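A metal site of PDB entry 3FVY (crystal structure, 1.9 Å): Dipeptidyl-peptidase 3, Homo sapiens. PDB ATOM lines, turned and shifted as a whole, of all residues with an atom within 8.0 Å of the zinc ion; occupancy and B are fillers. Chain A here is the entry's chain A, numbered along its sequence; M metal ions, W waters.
A ring nitrogen (NE2) of His 457 binds the zinc ion (2.0 Å).
The zinc ion is bound by OE2 of Glu 510 (2.1 Å).
NE2 of His 452 is bound to the zinc ion (2.1 Å).
Water W2 is bound to the zinc ion (2.4 Å).
Slightly farther from the zinc ion lies water W1 (2.6 Å).
Merely in contact with the zinc ion: Glu 453.
Of the 13 residues printed, 4 come within 4 Å of the zinc ion.
The side-chain carboxylate (OE2) of Glu 509 lies within hydrogen-bond range of a ring nitrogen (ND1) of His 457 (2.9 Å).
The side-chain carboxylate of Glu 510 sits close to a ring nitrogen (NE2) of His 570, at 3.4 Å.
A ring nitrogen (ND1) of His 452 lies within hydrogen-bond range of the side-chain carboxylate (OE1) of Glu 514 (2.8 Å).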
ATOM      1  N   PHE A 375     -20.783 -18.001  -6.486  1.00  0.00           N
ATOM      2  CA  PHE A 375     -21.007 -16.646  -6.946  1.00  0.00           C
ATOM      3  C   PHE A 375     -20.515 -15.688  -5.885  1.00  0.00           C
ATOM      4  O   PHE A 375     -20.890 -15.803  -4.722  1.00  0.00           O
ATOM      5  CB  PHE A 375     -22.503 -16.390  -7.240  1.00  0.00           C
ATOM      6  CG  PHE A 375     -22.821 -14.956  -7.520  1.00  0.00           C
ATOM      7  CD1 PHE A 375     -22.431 -14.361  -8.732  1.00  0.00           C
ATOM      8  CD2 PHE A 375     -23.501 -14.178  -6.581  1.00  0.00           C
ATOM      9  CE1 PHE A 375     -22.721 -13.038  -9.005  1.00  0.00           C
ATOM     10  CE2 PHE A 375     -23.795 -12.833  -6.850  1.00  0.00           C
ATOM     11  CZ  PHE A 375     -23.399 -12.273  -8.063  1.00  0.00           C
ATOM     12  N   VAL A 449     -30.635 -10.196  -8.977  1.00  0.00           N
ATOM     13  CA  VAL A 449     -29.326 -10.843  -8.903  1.00  0.00           C
ATOM     14  C   VAL A 449     -29.267 -12.048  -7.959  1.00  0.00           C
ATOM     15  O   VAL A 449     -28.756 -13.120  -8.326  1.00  0.00           O
ATOM     16  CB  VAL A 449     -28.240  -9.811  -8.489  1.00  0.00           C
ATOM     17  CG1 VAL A 449     -26.902 -10.534  -8.189  1.00  0.00           C
ATOM     18  CG2 VAL A 449     -28.075  -8.795  -9.610  1.00  0.00           C
ATOM     19  N   HIS A 452     -31.406 -14.928  -9.344  1.00  0.00           N
ATOM     20  CA  HIS A 452     -30.786 -15.422 -10.570  1.00  0.00           C
ATOM     21  C   HIS A 452     -29.575 -16.305 -10.253  1.00  0.00           C
ATOM     22  O   HIS A 452     -29.436 -17.397 -10.808  1.00  0.00           O
ATOM     23  CB  HIS A 452     -30.366 -14.206 -11.424  1.00  0.00           C
ATOM     24  CG  HIS A 452     -29.457 -14.510 -12.572  1.00  0.00           C
ATOM     25  ND1 HIS A 452     -29.762 -14.159 -13.867  1.00  0.00           N
ATOM     26  CD2 HIS A 452     -28.217 -15.066 -12.615  1.00  0.00           C
ATOM     27  CE1 HIS A 452     -28.758 -14.489 -14.664  1.00  0.00           C
ATOM     28  NE2 HIS A 452     -27.817 -15.049 -13.931  1.00  0.00           N
ATOM     29  N   GLU A 453     -28.712 -15.826  -9.354  1.00  0.00           N
ATOM     30  CA  GLU A 453     -27.441 -16.488  -9.108  1.00  0.00           C
ATOM     31  C   GLU A 453     -27.592 -17.692  -8.211  1.00  0.00           C
ATOM     32  O   GLU A 453     -26.937 -18.707  -8.439  1.00  0.00           O
ATOM     33  CB  GLU A 453     -26.428 -15.512  -8.510  1.00  0.00           C
ATOM     34  CG  GLU A 453     -26.015 -14.398  -9.468  1.00  0.00           C
ATOM     35  CD  GLU A 453     -25.202 -14.906 -10.653  1.00  0.00           C
ATOM     36  OE1 GLU A 453     -24.710 -16.062 -10.653  1.00  0.00           O
ATOM     37  OE2 GLU A 453     -25.033 -14.109 -11.597  1.00  0.00           O
ATOM     38  N   GLY A 456     -31.648 -19.514  -9.445  1.00  0.00           N
ATOM     39  CA  GLY A 456     -31.645 -19.688 -10.906  1.00  0.00           C
ATOM     40  C   GLY A 456     -30.603 -20.726 -11.254  1.00  0.00           C
ATOM     41  O   GLY A 456     -30.947 -21.899 -11.476  1.00  0.00           O
ATOM     42  N   HIS A 457     -29.329 -20.333 -11.234  1.00  0.00           N
ATOM     43  CA  HIS A 457     -28.245 -21.264 -11.547  1.00  0.00           C
ATOM     44  C   HIS A 457     -28.111 -22.443 -10.565  1.00  0.00           C
ATOM     45  O   HIS A 457     -27.575 -23.483 -10.935  1.00  0.00           O
ATOM     46  CB  HIS A 457     -26.898 -20.526 -11.648  1.00  0.00           C
ATOM     47  CG  HIS A 457     -26.804 -19.569 -12.794  1.00  0.00           C
ATOM     48  ND1 HIS A 457     -27.215 -19.885 -14.064  1.00  0.00           N
ATOM     49  CD2 HIS A 457     -26.327 -18.299 -12.851  1.00  0.00           C
ATOM     50  CE1 HIS A 457     -26.990 -18.856 -14.865  1.00  0.00           C
ATOM     51  NE2 HIS A 457     -26.450 -17.885 -14.149  1.00  0.00           N
ATOM     52  N   SER A 506     -25.288 -21.387 -23.338  1.00  0.00           N
ATOM     53  CA  SER A 506     -25.021 -20.310 -22.391  1.00  0.00           C
ATOM     54  C   SER A 506     -26.203 -19.310 -22.316  1.00  0.00           C
ATOM     55  O   SER A 506     -26.603 -18.874 -21.225  1.00  0.00           O
ATOM     56  CB  SER A 506     -23.660 -19.647 -22.700  1.00  0.00           C
ATOM     57  OG  SER A 506     -23.620 -18.341 -22.154  1.00  0.00           O
ATOM     58  N   GLU A 509     -29.368 -20.982 -20.663  1.00  0.00           N
ATOM     59  CA  GLU A 509     -29.196 -21.072 -19.196  1.00  0.00           C
ATOM     60  C   GLU A 509     -29.358 -19.707 -18.490  1.00  0.00           C
ATOM     61  O   GLU A 509     -29.924 -19.622 -17.387  1.00  0.00           O
ATOM     62  CB  GLU A 509     -27.868 -21.754 -18.833  1.00  0.00           C
ATOM     63  CG  GLU A 509     -27.532 -21.821 -17.298  1.00  0.00           C
ATOM     64  CD  GLU A 509     -28.647 -22.394 -16.420  1.00  0.00           C
ATOM     65  OE1 GLU A 509     -29.554 -23.123 -16.916  1.00  0.00           O
ATOM     66  OE2 GLU A 509     -28.625 -22.102 -15.194  1.00  0.00           O
ATOM     67  N   GLU A 510     -28.854 -18.651 -19.106  1.00  0.00           N
ATOM     68  CA  GLU A 510     -29.023 -17.325 -18.524  1.00  0.00           C
ATOM     69  C   GLU A 510     -30.506 -16.926 -18.575  1.00  0.00           C
ATOM     70  O   GLU A 510     -31.027 -16.313 -17.636  1.00  0.00           O
ATOM     71  CB  GLU A 510     -28.158 -16.271 -19.244  1.00  0.00           C
ATOM     72  CG  GLU A 510     -26.653 -16.512 -19.146  1.00  0.00           C
ATOM     73  CD  GLU A 510     -26.162 -16.617 -17.706  1.00  0.00           C
ATOM     74  OE1 GLU A 510     -25.184 -17.359 -17.450  1.00  0.00           O
ATOM     75  OE2 GLU A 510     -26.755 -15.981 -16.821  1.00  0.00           O
ATOM     76  N   CYS A 511     -31.164 -17.284 -19.680  1.00  0.00           N
ATOM     77  CA  CYS A 511     -32.601 -17.076 -19.815  1.00  0.00           C
ATOM     78  C   CYS A 511     -33.367 -17.760 -18.692  1.00  0.00           C
ATOM     79  O   CYS A 511     -34.262 -17.164 -18.071  1.00  0.00           O
ATOM     80  CB  CYS A 511     -33.091 -17.556 -21.193  1.00  0.00           C
ATOM     81  SG  CYS A 511     -34.795 -17.056 -21.564  1.00  0.00           S
ATOM     82  N   ALA A 513     -32.242 -18.818 -15.754  1.00  0.00           N
ATOM     83  CA  ALA A 513     -31.918 -18.151 -14.483  1.00  0.00           C
ATOM     84  C   ALA A 513     -32.578 -16.782 -14.305  1.00  0.00           C
ATOM     85  O   ALA A 513     -33.075 -16.486 -13.220  1.00  0.00           O
ATOM     86  CB  ALA A 513     -30.414 -18.036 -14.313  1.00  0.00           C
ATOM     87  N   GLU A 514     -32.579 -15.959 -15.356  1.00  0.00           N
ATOM     88  CA  GLU A 514     -33.298 -14.666 -15.336  1.00  0.00           C
ATOM     89  C   GLU A 514     -34.799 -14.873 -15.121  1.00  0.00           C
ATOM     90  O   GLU A 514     -35.440 -14.129 -14.389  1.00  0.00           O
ATOM     91  CB  GLU A 514     -33.038 -13.864 -16.619  1.00  0.00           C
ATOM     92  CG  GLU A 514     -31.613 -13.285 -16.735  1.00  0.00           C
ATOM     93  CD  GLU A 514     -31.389 -12.052 -15.849  1.00  0.00           C
ATOM     94  OE1 GLU A 514     -31.487 -12.147 -14.614  1.00  0.00           O
ATOM     95  OE2 GLU A 514     -31.074 -10.979 -16.419  1.00  0.00           O
ATOM     96  N   HIS A 570     -26.376 -13.150 -22.975  1.00  0.00           N
ATOM     97  CA  HIS A 570     -27.267 -12.519 -21.993  1.00  0.00           C
ATOM     98  C   HIS A 570     -28.332 -11.659 -22.660  1.00  0.00           C
ATOM     99  O   HIS A 570     -29.489 -11.627 -22.228  1.00  0.00           O
ATOM    100  CB  HIS A 570     -26.486 -11.623 -21.025  1.00  0.00           C
ATOM    101  CG  HIS A 570     -25.760 -12.359 -19.941  1.00  0.00           C
ATOM    102  ND1 HIS A 570     -24.496 -12.893 -20.115  1.00  0.00           N
ATOM    103  CD2 HIS A 570     -26.101 -12.604 -18.650  1.00  0.00           C
ATOM    104  CE1 HIS A 570     -24.105 -13.453 -18.991  1.00  0.00           C
ATOM    105  NE2 HIS A 570     -25.058 -13.289 -18.081  1.00  0.00           N
HETATM  106 ZN    ZN M   1     -26.204 -15.971 -14.834  1.00  0.00          ZN
HETATM  107  O   HOH W   1     -25.044 -13.654 -15.244  1.00  0.00           O
HETATM  108  O   HOH W   2     -24.089 -15.230 -14.016  1.00  0.00           O
